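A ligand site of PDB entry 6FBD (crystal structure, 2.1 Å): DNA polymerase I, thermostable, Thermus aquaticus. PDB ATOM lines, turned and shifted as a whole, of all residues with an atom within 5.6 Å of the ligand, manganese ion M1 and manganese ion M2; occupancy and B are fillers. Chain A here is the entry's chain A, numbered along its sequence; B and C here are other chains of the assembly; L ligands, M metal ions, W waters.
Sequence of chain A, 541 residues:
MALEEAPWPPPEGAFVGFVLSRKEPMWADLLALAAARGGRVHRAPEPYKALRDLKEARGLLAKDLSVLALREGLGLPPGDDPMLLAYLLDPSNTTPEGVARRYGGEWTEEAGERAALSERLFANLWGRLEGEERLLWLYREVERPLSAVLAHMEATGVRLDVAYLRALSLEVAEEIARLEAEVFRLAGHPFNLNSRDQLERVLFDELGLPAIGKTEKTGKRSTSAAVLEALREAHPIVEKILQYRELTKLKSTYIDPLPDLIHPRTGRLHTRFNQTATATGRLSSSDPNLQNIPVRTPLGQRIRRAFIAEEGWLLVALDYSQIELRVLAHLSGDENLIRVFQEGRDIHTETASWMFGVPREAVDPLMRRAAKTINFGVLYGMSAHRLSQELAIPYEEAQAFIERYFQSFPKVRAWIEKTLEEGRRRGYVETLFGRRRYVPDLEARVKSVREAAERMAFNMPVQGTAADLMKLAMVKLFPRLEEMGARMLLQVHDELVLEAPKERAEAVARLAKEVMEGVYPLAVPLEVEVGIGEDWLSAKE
Residues that only touch manganese ion M1: Glu 495. Within 4 Å of manganese ion M1: Asp 319, Asp 494, Glu 495 and DC 12 of chain B. The nearest printed residue that does not touch manganese ion M1 is Lys 540 (4.1 Å).
The side-chain carboxylate of Glu 495 is in salt-bridge range of the side-chain amino group of Lys 540 (3.0 Å). OP2 of DC 12 of chain B lies within salt-bridge range of NH2 of Arg 369, 2.8 Å away. OE2 of Glu 324 is in salt-bridge range of NH2 of Arg 282 (3.9 Å). O2 of DC 12 of chain B sits close to N2 of DG 5 of chain C, at 2.6 Å. The side-chain carboxylate (OD2) of Asp 346 is in salt-bridge range of the guanidinium group (NH2) of Arg 368, 2.9 Å away. O2 of DC 12 of chain B is in hydrogen-bond range of NH1 of Arg 282 (2.7 Å). The side-chain carboxylate (OD2) of Asp 319 sits close to the side-chain amino group (NZ) of Lys 540 (3.5 Å). N2 of DG 5 of chain C sits at hydrogen-bond distance from the guanidinium group of Arg 282, at 3.3 Å.
Three residues have an atom within 4 Å of manganese ion M2: Asp 319, Tyr 320 and Asp 494.
Manganese ion M2 is bound by the backbone carbonyl oxygen (O) of Tyr 320, at 2.1 Å. OD2 of Asp 494 binds manganese ion M2 (2.1 Å). Manganese ion M2 is bound by the side-chain carboxylate (OD1) of Asp 319 (2.1 Å). An oxygen (O10) of the ligand is bound to manganese ion M2 (2.1 Å). An oxygen (O3) of the ligand binds manganese ion M2 (2.2 Å). O2 of the ligand binds manganese ion M2 (2.3 Å). Manganese ion M2 has six donor atoms within binding distance.
O6 of the ligand lies within hydrogen-bond range of NE2 of His 348, 2.8 Å away. An oxygen (O3) of the ligand sits close to the backbone NH (N) of Ile 323 (3.4 Å). The guanidinium group (NH1) of Arg 368 lies within salt-bridge range of an oxygen (O7) of the ligand (2.6 Å). N of Glu 324 sits at hydrogen-bond distance from O8 of the ligand (3.3 Å). N3 of DG 5 of chain C sits close to a nitrogen (N2) of the ligand (3.3 Å). O2 of DC 4 of chain C sits at hydrogen-bond distance from N2 of the ligand. NZ of Lys 372 lies within hydrogen-bond range of N4 of the ligand (3.3 Å). An oxygen (O11) of the ligand lies within hydrogen-bond range of the guanidinium group (NH2) of Arg 282. O9 of the ligand is in hydrogen-bond range of N of Gln 322, at 3.3 Å.
Manganese ion M1 is bound by water W1, O2 of the ligand, OD1 of Asp 494, water W3, OD2 of Asp 319 and O3' of DC 12 of chain B. Manganese ion M1 has six donor atoms within binding distance.
Water W1 bridges O5 of the ligand and NZ of Lys 540.
CA of Ser 321 touches O4 of the ligand (3.6 Å). CG2 of Thr 373 touches O1 of the ligand, 3.9 Å away. CZ of Phe 376 touches O8 of the ligand, at 3.1 Å. Tyr 380 touches the ligand. Hydrophobic or aromatic side chains within 4 Å of the ligand: Ile 323, His 348, Phe 376 and Tyr 380.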
ATOM      1  N   ARG A 282     -29.972  -2.693   5.906  1.00  0.00           N
ATOM      2  CA  ARG A 282     -30.746  -3.258   7.003  1.00  0.00           C
ATOM      3  C   ARG A 282     -32.006  -3.917   6.467  1.00  0.00           C
ATOM      4  O   ARG A 282     -32.471  -3.634   5.360  1.00  0.00           O
ATOM      5  CB  ARG A 282     -31.138  -2.175   8.003  1.00  0.00           C
ATOM      6  CG  ARG A 282     -30.045  -1.776   8.980  1.00  0.00           C
ATOM      7  CD  ARG A 282     -30.658  -0.921  10.065  1.00  0.00           C
ATOM      8  NE  ARG A 282     -29.792  -0.777  11.218  1.00  0.00           N
ATOM      9  CZ  ARG A 282     -30.143  -0.124  12.324  1.00  0.00           C
ATOM     10  NH1 ARG A 282     -31.346   0.440  12.410  1.00  0.00           N
ATOM     11  NH2 ARG A 282     -29.291  -0.026  13.333  1.00  0.00           N
ATOM     12  N   ASP A 319     -27.736 -10.374  21.319  1.00  0.00           N
ATOM     13  CA  ASP A 319     -27.602  -8.993  20.875  1.00  0.00           C
ATOM     14  C   ASP A 319     -26.124  -8.633  20.836  1.00  0.00           C
ATOM     15  O   ASP A 319     -25.395  -8.867  21.807  1.00  0.00           O
ATOM     16  CB  ASP A 319     -28.365  -8.048  21.809  1.00  0.00           C
ATOM     17  CG  ASP A 319     -28.413  -6.623  21.291  1.00  0.00           C
ATOM     18  OD1 ASP A 319     -27.344  -6.046  21.021  1.00  0.00           O
ATOM     19  OD2 ASP A 319     -29.541  -6.095  21.137  1.00  0.00           O
ATOM     20  N   TYR A 320     -25.678  -8.064  19.720  1.00  0.00           N
ATOM     21  CA  TYR A 320     -24.283  -7.661  19.594  1.00  0.00           C
ATOM     22  C   TYR A 320     -23.998  -6.475  20.492  1.00  0.00           C
ATOM     23  O   TYR A 320     -24.823  -5.562  20.642  1.00  0.00           O
ATOM     24  CB  TYR A 320     -23.945  -7.305  18.146  1.00  0.00           C
ATOM     25  CG  TYR A 320     -23.745  -8.484  17.203  1.00  0.00           C
ATOM     26  CD1 TYR A 320     -22.576  -9.248  17.247  1.00  0.00           C
ATOM     27  CD2 TYR A 320     -24.707  -8.810  16.259  1.00  0.00           C
ATOM     28  CE1 TYR A 320     -22.395 -10.312  16.381  1.00  0.00           C
ATOM     29  CE2 TYR A 320     -24.529  -9.864  15.392  1.00  0.00           C
ATOM     30  CZ  TYR A 320     -23.369 -10.609  15.454  1.00  0.00           C
ATOM     31  OH  TYR A 320     -23.201 -11.657  14.575  1.00  0.00           O
ATOM     32  N   SER A 321     -22.806  -6.481  21.088  1.00  0.00           N
ATOM     33  CA  SER A 321     -22.386  -5.421  21.993  1.00  0.00           C
ATOM     34  C   SER A 321     -21.774  -4.277  21.193  1.00  0.00           C
ATOM     35  O   SER A 321     -20.871  -4.490  20.386  1.00  0.00           O
ATOM     36  CB  SER A 321     -21.379  -5.956  23.009  1.00  0.00           C
ATOM     37  OG  SER A 321     -20.942  -4.944  23.898  1.00  0.00           O
ATOM     38  N   GLN A 322     -22.282  -3.064  21.417  1.00  0.00           N
ATOM     39  CA  GLN A 322     -21.697  -1.837  20.866  1.00  0.00           C
ATOM     40  C   GLN A 322     -21.317  -2.045  19.403  1.00  0.00           C
ATOM     41  O   GLN A 322     -20.215  -1.712  18.960  1.00  0.00           O
ATOM     42  CB  GLN A 322     -20.481  -1.401  21.682  1.00  0.00           C
ATOM     43  CG  GLN A 322     -20.658  -1.558  23.187  1.00  0.00           C
ATOM     44  CD  GLN A 322     -19.390  -1.266  23.965  1.00  0.00           C
ATOM     45  OE1 GLN A 322     -18.968  -2.064  24.797  1.00  0.00           O
ATOM     46  NE2 GLN A 322     -18.786  -0.119  23.683  1.00  0.00           N
ATOM     47  N   ILE A 323     -22.259  -2.604  18.639  1.00  0.00           N
ATOM     48  CA  ILE A 323     -21.896  -3.233  17.362  1.00  0.00           C
ATOM     49  C   ILE A 323     -21.240  -2.221  16.430  1.00  0.00           C
ATOM     50  O   ILE A 323     -20.125  -2.442  15.937  1.00  0.00           O
ATOM     51  CB  ILE A 323     -23.121  -3.911  16.720  1.00  0.00           C
ATOM     52  CG1 ILE A 323     -22.770  -4.478  15.339  1.00  0.00           C
ATOM     53  CG2 ILE A 323     -24.316  -2.969  16.629  1.00  0.00           C
ATOM     54  CD1 ILE A 323     -21.637  -5.485  15.359  1.00  0.00           C
ATOM     55  N   GLU A 324     -21.908  -1.101  16.169  1.00  0.00           N
ATOM     56  CA  GLU A 324     -21.391  -0.156  15.182  1.00  0.00           C
ATOM     57  C   GLU A 324     -20.079   0.492  15.627  1.00  0.00           C
ATOM     58  O   GLU A 324     -19.293   0.911  14.778  1.00  0.00           O
ATOM     59  CB  GLU A 324     -22.444   0.906  14.861  1.00  0.00           C
ATOM     60  CG  GLU A 324     -23.600   0.361  14.016  1.00  0.00           C
ATOM     61  CD  GLU A 324     -24.497   1.429  13.408  1.00  0.00           C
ATOM     62  OE1 GLU A 324     -24.136   2.629  13.436  1.00  0.00           O
ATOM     63  OE2 GLU A 324     -25.576   1.056  12.900  1.00  0.00           O
ATOM     64  N   LEU A 325     -19.823   0.557  16.934  1.00  0.00           N
ATOM     65  CA  LEU A 325     -18.533   1.063  17.397  1.00  0.00           C
ATOM     66  C   LEU A 325     -17.410   0.081  17.068  1.00  0.00           C
ATOM     67  O   LEU A 325     -16.308   0.491  16.665  1.00  0.00           O
ATOM     68  CB  LEU A 325     -18.561   1.349  18.892  1.00  0.00           C
ATOM     69  CG  LEU A 325     -19.378   2.559  19.364  1.00  0.00           C
ATOM     70  CD1 LEU A 325     -19.288   2.694  20.884  1.00  0.00           C
ATOM     71  CD2 LEU A 325     -18.908   3.848  18.689  1.00  0.00           C
ATOM     72  N   ASP A 346     -16.551  -0.558  28.075  1.00  0.00           N
ATOM     73  CA  ASP A 346     -17.894  -0.266  27.580  1.00  0.00           C
ATOM     74  C   ASP A 346     -18.052   1.239  27.478  1.00  0.00           C
ATOM     75  O   ASP A 346     -18.032   1.946  28.498  1.00  0.00           O
ATOM     76  CB  ASP A 346     -18.955  -0.867  28.503  1.00  0.00           C
ATOM     77  CG  ASP A 346     -20.347  -0.806  27.911  1.00  0.00           C
ATOM     78  OD1 ASP A 346     -20.639   0.164  27.182  1.00  0.00           O
ATOM     79  OD2 ASP A 346     -21.133  -1.737  28.177  1.00  0.00           O
ATOM     80  N   HIS A 348     -20.739   2.883  26.227  1.00  0.00           N
ATOM     81  CA  HIS A 348     -22.075   3.305  26.647  1.00  0.00           C
ATOM     82  C   HIS A 348     -22.126   3.522  28.159  1.00  0.00           C
ATOM     83  O   HIS A 348     -22.629   4.544  28.631  1.00  0.00           O
ATOM     84  CB  HIS A 348     -23.117   2.259  26.227  1.00  0.00           C
ATOM     85  CG  HIS A 348     -23.268   2.129  24.747  1.00  0.00           C
ATOM     86  ND1 HIS A 348     -22.722   3.028  23.858  1.00  0.00           N
ATOM     87  CD2 HIS A 348     -23.915   1.200  23.992  1.00  0.00           C
ATOM     88  CE1 HIS A 348     -23.025   2.661  22.628  1.00  0.00           C
ATOM     89  NE2 HIS A 348     -23.739   1.558  22.677  1.00  0.00           N
ATOM     90  N   ARG A 368     -28.065   3.769  30.838  1.00  0.00           N
ATOM     91  CA  ARG A 368     -27.204   3.313  29.742  1.00  0.00           C
ATOM     92  C   ARG A 368     -27.870   3.529  28.386  1.00  0.00           C
ATOM     93  O   ARG A 368     -27.194   3.863  27.407  1.00  0.00           O
ATOM     94  CB  ARG A 368     -26.842   1.845  29.942  1.00  0.00           C
ATOM     95  CG  ARG A 368     -25.780   1.354  28.975  1.00  0.00           C
ATOM     96  CD  ARG A 368     -25.215   0.004  29.384  1.00  0.00           C
ATOM     97  NE  ARG A 368     -24.232  -0.478  28.423  1.00  0.00           N
ATOM     98  CZ  ARG A 368     -24.526  -1.148  27.321  1.00  0.00           C
ATOM     99  NH1 ARG A 368     -25.783  -1.444  27.024  1.00  0.00           N
ATOM    100  NH2 ARG A 368     -23.555  -1.540  26.509  1.00  0.00           N
ATOM    101  N   ARG A 369     -29.188   3.334  28.309  1.00  0.00           N
ATOM    102  CA  ARG A 369     -29.906   3.648  27.075  1.00  0.00           C
ATOM    103  C   ARG A 369     -29.686   5.100  26.676  1.00  0.00           C
ATOM    104  O   ARG A 369     -29.284   5.404  25.556  1.00  0.00           O
ATOM    105  CB  ARG A 369     -31.398   3.365  27.232  1.00  0.00           C
ATOM    106  CG  ARG A 369     -31.754   1.911  27.443  1.00  0.00           C
ATOM    107  CD  ARG A 369     -33.260   1.711  27.352  1.00  0.00           C
ATOM    108  NE  ARG A 369     -33.774   2.124  26.052  1.00  0.00           N
ATOM    109  CZ  ARG A 369     -33.709   1.395  24.946  1.00  0.00           C
ATOM    110  NH1 ARG A 369     -33.150   0.183  24.965  1.00  0.00           N
ATOM    111  NH2 ARG A 369     -34.196   1.869  23.802  1.00  0.00           N
ATOM    112  N   LYS A 372     -26.428   5.610  25.284  1.00  0.00           N
ATOM    113  CA  LYS A 372     -26.241   5.028  23.955  1.00  0.00           C
ATOM    114  C   LYS A 372     -26.652   6.010  22.858  1.00  0.00           C
ATOM    115  O   LYS A 372     -25.937   6.166  21.858  1.00  0.00           O
ATOM    116  CB  LYS A 372     -27.034   3.723  23.849  1.00  0.00           C
ATOM    117  CG  LYS A 372     -27.009   3.110  22.470  1.00  0.00           C
ATOM    118  CD  LYS A 372     -28.249   3.484  21.667  1.00  0.00           C
ATOM    119  CE  LYS A 372     -29.424   2.589  22.024  1.00  0.00           C
ATOM    120  NZ  LYS A 372     -30.731   3.226  21.663  1.00  0.00           N
ATOM    121  N   THR A 373     -27.796   6.671  23.034  1.00  0.00           N
ATOM    122  CA  THR A 373     -28.222   7.667  22.056  1.00  0.00           C
ATOM    123  C   THR A 373     -27.189   8.786  21.924  1.00  0.00           C
ATOM    124  O   THR A 373     -26.906   9.255  20.820  1.00  0.00           O
ATOM    125  CB  THR A 373     -29.581   8.247  22.449  1.00  0.00           C
ATOM    126  OG1 THR A 373     -30.476   7.170  22.748  1.00  0.00           O
ATOM    127  CG2 THR A 373     -30.157   9.093  21.324  1.00  0.00           C
ATOM    128  N   PHE A 376     -23.990   7.617  19.834  1.00  0.00           N
ATOM    129  CA  PHE A 376     -24.223   7.550  18.400  1.00  0.00           C
ATOM    130  C   PHE A 376     -24.694   8.887  17.846  1.00  0.00           C
ATOM    131  O   PHE A 376     -24.406   9.206  16.684  1.00  0.00           O
ATOM    132  CB  PHE A 376     -25.244   6.444  18.087  1.00  0.00           C
ATOM    133  CG  PHE A 376     -24.735   5.059  18.394  1.00  0.00           C
ATOM    134  CD1 PHE A 376     -23.642   4.546  17.708  1.00  0.00           C
ATOM    135  CD2 PHE A 376     -25.342   4.274  19.362  1.00  0.00           C
ATOM    136  CE1 PHE A 376     -23.165   3.275  17.987  1.00  0.00           C
ATOM    137  CE2 PHE A 376     -24.864   3.004  19.642  1.00  0.00           C
ATOM    138  CZ  PHE A 376     -23.775   2.509  18.944  1.00  0.00           C
ATOM    139  N   GLY A 377     -25.405   9.680  18.639  1.00  0.00           N
ATOM    140  CA  GLY A 377     -25.739  11.025  18.201  1.00  0.00           C
ATOM    141  C   GLY A 377     -24.508  11.847  17.896  1.00  0.00           C
ATOM    142  O   GLY A 377     -24.357  12.391  16.808  1.00  0.00           O
ATOM    143  N   TYR A 380     -22.435  10.571  14.676  1.00  0.00           N
ATOM    144  CA  TYR A 380     -22.948  10.771  13.328  1.00  0.00           C
ATOM    145  C   TYR A 380     -23.338  12.213  13.032  1.00  0.00           C
ATOM    146  O   TYR A 380     -24.073  12.457  12.069  1.00  0.00           O
ATOM    147  CB  TYR A 380     -24.142   9.838  13.083  1.00  0.00           C
ATOM    148  CG  TYR A 380     -23.752   8.373  13.064  1.00  0.00           C
ATOM    149  CD1 TYR A 380     -22.864   7.884  12.116  1.00  0.00           C
ATOM    150  CD2 TYR A 380     -24.284   7.482  13.987  1.00  0.00           C
ATOM    151  CE1 TYR A 380     -22.502   6.546  12.091  1.00  0.00           C
ATOM    152  CE2 TYR A 380     -23.934   6.141  13.969  1.00  0.00           C
ATOM    153  CZ  TYR A 380     -23.045   5.683  13.021  1.00  0.00           C
ATOM    154  OH  TYR A 380     -22.686   4.356  12.995  1.00  0.00           O
ATOM    155  N   ASN A 459     -22.436   7.371   7.474  1.00  0.00           N
ATOM    156  CA  ASN A 459     -23.159   6.439   8.342  1.00  0.00           C
ATOM    157  C   ASN A 459     -23.392   5.096   7.668  1.00  0.00           C
ATOM    158  O   ASN A 459     -23.409   4.060   8.342  1.00  0.00           O
ATOM    159  CB  ASN A 459     -24.498   7.038   8.768  1.00  0.00           C
ATOM    160  CG  ASN A 459     -25.436   5.991   9.374  1.00  0.00           C
ATOM    161  OD1 ASN A 459     -26.149   5.285   8.654  1.00  0.00           O
ATOM    162  ND2 ASN A 459     -25.428   5.888  10.699  1.00  0.00           N
ATOM    163  N   VAL A 492     -33.741  -7.932  15.034  1.00  0.00           N
ATOM    164  CA  VAL A 492     -33.897  -6.496  15.279  1.00  0.00           C
ATOM    165  C   VAL A 492     -32.561  -5.827  15.016  1.00  0.00           C
ATOM    166  O   VAL A 492     -31.931  -5.279  15.937  1.00  0.00           O
ATOM    167  CB  VAL A 492     -34.419  -6.218  16.694  1.00  0.00           C
ATOM    168  CG1 VAL A 492     -35.082  -4.854  16.755  1.00  0.00           C
ATOM    169  CG2 VAL A 492     -35.392  -7.298  17.142  1.00  0.00           C
ATOM    170  N   ASP A 494     -29.406  -5.754  15.147  1.00  0.00           N
ATOM    171  CA  ASP A 494     -28.204  -6.301  15.752  1.00  0.00           C
ATOM    172  C   ASP A 494     -28.530  -7.374  16.786  1.00  0.00           C
ATOM    173  O   ASP A 494     -27.704  -7.659  17.664  1.00  0.00           O
ATOM    174  CB  ASP A 494     -27.358  -5.194  16.389  1.00  0.00           C
ATOM    175  CG  ASP A 494     -27.790  -4.900  17.810  1.00  0.00           C
ATOM    176  OD1 ASP A 494     -29.009  -4.935  18.085  1.00  0.00           O
ATOM    177  OD2 ASP A 494     -26.912  -4.658  18.659  1.00  0.00           O
ATOM    178  N   GLU A 495     -29.713  -7.957  16.700  1.00  0.00           N
ATOM    179  CA  GLU A 495     -30.221  -8.877  17.708  1.00  0.00           C
ATOM    180  C   GLU A 495     -31.027  -9.976  17.017  1.00  0.00           C
ATOM    181  O   GLU A 495     -31.580  -9.769  15.937  1.00  0.00           O
ATOM    182  CB  GLU A 495     -31.096  -8.128  18.726  1.00  0.00           C
ATOM    183  CG  GLU A 495     -31.975  -8.990  19.625  1.00  0.00           C
ATOM    184  CD  GLU A 495     -32.945  -8.167  20.451  1.00  0.00           C
ATOM    185  OE1 GLU A 495     -32.901  -6.926  20.339  1.00  0.00           O
ATOM    186  OE2 GLU A 495     -33.742  -8.764  21.199  1.00  0.00           O
ATOM    187  N   LYS A 540     -33.784 -11.059  27.733  1.00  0.00           N
ATOM    188  CA  LYS A 540     -32.814 -10.012  27.428  1.00  0.00           C
ATOM    189  C   LYS A 540     -32.326  -9.305  28.686  1.00  0.00           C
ATOM    190  O   LYS A 540     -31.775  -8.202  28.598  1.00  0.00           O
ATOM    191  CB  LYS A 540     -33.423  -9.009  26.447  1.00  0.00           C
ATOM    192  CG  LYS A 540     -32.438  -8.502  25.400  1.00  0.00           C
ATOM    193  CD  LYS A 540     -33.041  -7.393  24.560  1.00  0.00           C
ATOM    194  CE  LYS A 540     -32.039  -6.836  23.567  1.00  0.00           C
ATOM    195  NZ  LYS A 540     -32.471  -5.541  22.990  1.00  0.00           N
ATOM    196  P    DC B  12     -34.346  -1.326  21.169  1.00  0.00           P
ATOM    197  OP1  DC B  12     -34.405  -2.698  21.718  1.00  0.00           O
ATOM    198  OP2  DC B  12     -33.845  -0.224  22.017  1.00  0.00           O
ATOM    199  O5'  DC B  12     -33.477  -1.326  19.823  1.00  0.00           O
ATOM    200  C5'  DC B  12     -33.478  -2.464  18.976  1.00  0.00           C
ATOM    201  C4'  DC B  12     -32.557  -2.248  17.790  1.00  0.00           C
ATOM    202  O4'  DC B  12     -33.076  -1.176  16.956  1.00  0.00           O
ATOM    203  C3'  DC B  12     -31.146  -1.838  18.154  1.00  0.00           C
ATOM    204  O3'  DC B  12     -30.319  -2.978  18.334  1.00  0.00           O
ATOM    205  C2'  DC B  12     -30.699  -0.969  16.983  1.00  0.00           C
ATOM    206  C1'  DC B  12     -32.008  -0.410  16.419  1.00  0.00           C
ATOM    207  N1   DC B  12     -32.246   1.029  16.760  1.00  0.00           N
ATOM    208  C2   DC B  12     -31.900   2.033  15.853  1.00  0.00           C
ATOM    209  O2   DC B  12     -31.393   1.712  14.771  1.00  0.00           O
ATOM    210  N3   DC B  12     -32.131   3.327  16.177  1.00  0.00           N
ATOM    211  C4   DC B  12     -32.682   3.630  17.353  1.00  0.00           C
ATOM    212  N4   DC B  12     -32.895   4.926  17.630  1.00  0.00           N
ATOM    213  C5   DC B  12     -33.045   2.624  18.298  1.00  0.00           C
ATOM    214  C6   DC B  12     -32.808   1.353  17.964  1.00  0.00           C
ATOM    215  P    DC C   4     -28.923  17.659  14.863  1.00  0.00           P
ATOM    216  OP1  DC C   4     -30.374  17.667  15.115  1.00  0.00           O
ATOM    217  OP2  DC C   4     -28.027  18.501  15.686  1.00  0.00           O
ATOM    218  O5'  DC C   4     -28.390  16.151  14.953  1.00  0.00           O
ATOM    219  C5'  DC C   4     -28.932  15.152  14.096  1.00  0.00           C
ATOM    220  C4'  DC C   4     -27.865  14.158  13.686  1.00  0.00           C
ATOM    221  O4'  DC C   4     -27.374  13.479  14.875  1.00  0.00           O
ATOM    222  C3'  DC C   4     -28.352  13.055  12.759  1.00  0.00           C
ATOM    223  O3'  DC C   4     -28.184  13.429  11.402  1.00  0.00           O
ATOM    224  C2'  DC C   4     -27.462  11.874  13.134  1.00  0.00           C
ATOM    225  C1'  DC C   4     -27.228  12.081  14.617  1.00  0.00           C
ATOM    226  N1   DC C   4     -28.180  11.331  15.491  1.00  0.00           N
ATOM    227  C2   DC C   4     -28.028   9.953  15.641  1.00  0.00           C
ATOM    228  O2   DC C   4     -27.105   9.384  15.047  1.00  0.00           O
ATOM    229  N3   DC C   4     -28.894   9.277  16.438  1.00  0.00           N
ATOM    230  C4   DC C   4     -29.870   9.926  17.063  1.00  0.00           C
ATOM    231  N4   DC C   4     -30.699   9.217  17.836  1.00  0.00           N
ATOM    232  C5   DC C   4     -30.044  11.339  16.918  1.00  0.00           C
ATOM    233  C6   DC C   4     -29.184  11.994  16.131  1.00  0.00           C
ATOM    234  P    DG C   5     -29.308  13.054  10.316  1.00  0.00           P
ATOM    235  OP1  DG C   5     -28.938  13.769   9.072  1.00  0.00           O
ATOM    236  OP2  DG C   5     -30.636  13.241  10.934  1.00  0.00           O
ATOM    237  O5'  DG C   5     -29.110  11.475  10.092  1.00  0.00           O
ATOM    238  C5'  DG C   5     -28.016  10.999   9.334  1.00  0.00           C
ATOM    239  C4'  DG C   5     -27.897   9.491   9.419  1.00  0.00           C
ATOM    240  O4'  DG C   5     -27.776   9.092  10.810  1.00  0.00           O
ATOM    241  C3'  DG C   5     -29.095   8.716   8.916  1.00  0.00           C
ATOM    242  O3'  DG C   5     -29.074   8.571   7.508  1.00  0.00           O
ATOM    243  C2'  DG C   5     -28.943   7.389   9.635  1.00  0.00           C
ATOM    244  C1'  DG C   5     -28.360   7.807  10.986  1.00  0.00           C
ATOM    245  N9   DG C   5     -29.366   7.871  12.041  1.00  0.00           N
ATOM    246  C8   DG C   5     -29.970   8.991  12.554  1.00  0.00           C
ATOM    247  N7   DG C   5     -30.834   8.734  13.497  1.00  0.00           N
ATOM    248  C5   DG C   5     -30.802   7.349  13.615  1.00  0.00           C
ATOM    249  C6   DG C   5     -31.522   6.479  14.473  1.00  0.00           C
ATOM    250  O6   DG C   5     -32.362   6.768  15.331  1.00  0.00           O
ATOM    251  N1   DG C   5     -31.179   5.144  14.251  1.00  0.00           N
ATOM    252  C2   DG C   5     -30.259   4.707  13.328  1.00  0.00           C
ATOM    253  N2   DG C   5     -30.063   3.380  13.262  1.00  0.00           N
ATOM    254  N3   DG C   5     -29.580   5.505  12.525  1.00  0.00           N
ATOM    255  C4   DG C   5     -29.897   6.805  12.722  1.00  0.00           C
HETATM  256  N1  LIG L   1     -28.924   6.421  16.760  1.00  0.00           N
HETATM  257  C1  LIG L   1     -28.137   5.848  15.805  1.00  0.00           C
HETATM  258  N2  LIG L   1     -27.618   6.652  14.882  1.00  0.00           N
HETATM  259  N3  LIG L   1     -27.867   4.545  15.762  1.00  0.00           N
HETATM  260  C2  LIG L   1     -28.466   3.857  16.751  1.00  0.00           C
HETATM  261  C3  LIG L   1     -29.286   4.340  17.752  1.00  0.00           C
HETATM  262  C4  LIG L   1     -29.555   5.748  17.783  1.00  0.00           C
HETATM  263  O1  LIG L   1     -30.244   6.352  18.614  1.00  0.00           O
HETATM  264  N4  LIG L   1     -29.704   3.308  18.576  1.00  0.00           N
HETATM  265  C5  LIG L   1     -29.130   2.242  18.077  1.00  0.00           C
HETATM  266  N5  LIG L   1     -28.356   2.503  16.974  1.00  0.00           N
HETATM  267  P1  LIG L   1     -28.397  -1.594  20.374  1.00  0.00           P
HETATM  268  P2  LIG L   1     -25.541  -1.289  21.056  1.00  0.00           P
HETATM  269  P3  LIG L   1     -25.479  -2.725  23.591  1.00  0.00           P
HETATM  270  C6  LIG L   1     -27.517   1.552  16.218  1.00  0.00           C
HETATM  271  O2  LIG L   1     -28.428  -3.054  20.441  1.00  0.00           O
HETATM  272  O3  LIG L   1     -25.266  -2.372  20.117  1.00  0.00           O
HETATM  273  O4  LIG L   1     -24.196  -3.267  24.211  1.00  0.00           O
HETATM  274  C7  LIG L   1     -26.057   1.564  16.658  1.00  0.00           C
HETATM  275  O5  LIG L   1     -29.719  -1.056  21.048  1.00  0.00           O
HETATM  276  O6  LIG L   1     -24.786   0.004  20.565  1.00  0.00           O
HETATM  277  O7  LIG L   1     -26.405  -2.107  24.591  1.00  0.00           O
HETATM  278  C8  LIG L   1     -25.987   0.386  17.624  1.00  0.00           C
HETATM  279  O8  LIG L   1     -24.668  -0.176  17.661  1.00  0.00           O
HETATM  280  N6  LIG L   1     -27.134  -0.966  21.186  1.00  0.00           N
HETATM  281  O9  LIG L   1     -25.014  -1.634  22.521  1.00  0.00           O
HETATM  282  O10 LIG L   1     -26.152  -3.835  22.772  1.00  0.00           O
HETATM  283  C9  LIG L   1     -26.967  -0.594  16.981  1.00  0.00           C
HETATM  284  O11 LIG L   1     -28.014   0.234  16.441  1.00  0.00           O
HETATM  285  C10 LIG L   1     -27.547  -1.637  17.897  1.00  0.00           C
HETATM  286  O12 LIG L   1     -28.338  -0.997  18.932  1.00  0.00           O
HETATM  287 MN    MN M   1     -29.953  -4.390  19.907  1.00  0.00          MN
HETATM  288 MN    MN M   2     -26.382  -4.168  20.661  1.00  0.00          MN
HETATM  289  O   HOH W   1     -30.871  -3.479  21.473  1.00  0.00           O
HETATM  290  O   HOH W   2     -25.748  -6.109  23.979  1.00  0.00           O
HETATM  291  O   HOH W   3     -31.849  -5.190  19.367  1.00  0.00           O
HETATM  292  O   HOH W   4     -27.943   0.415  24.047  1.00  0.00           O
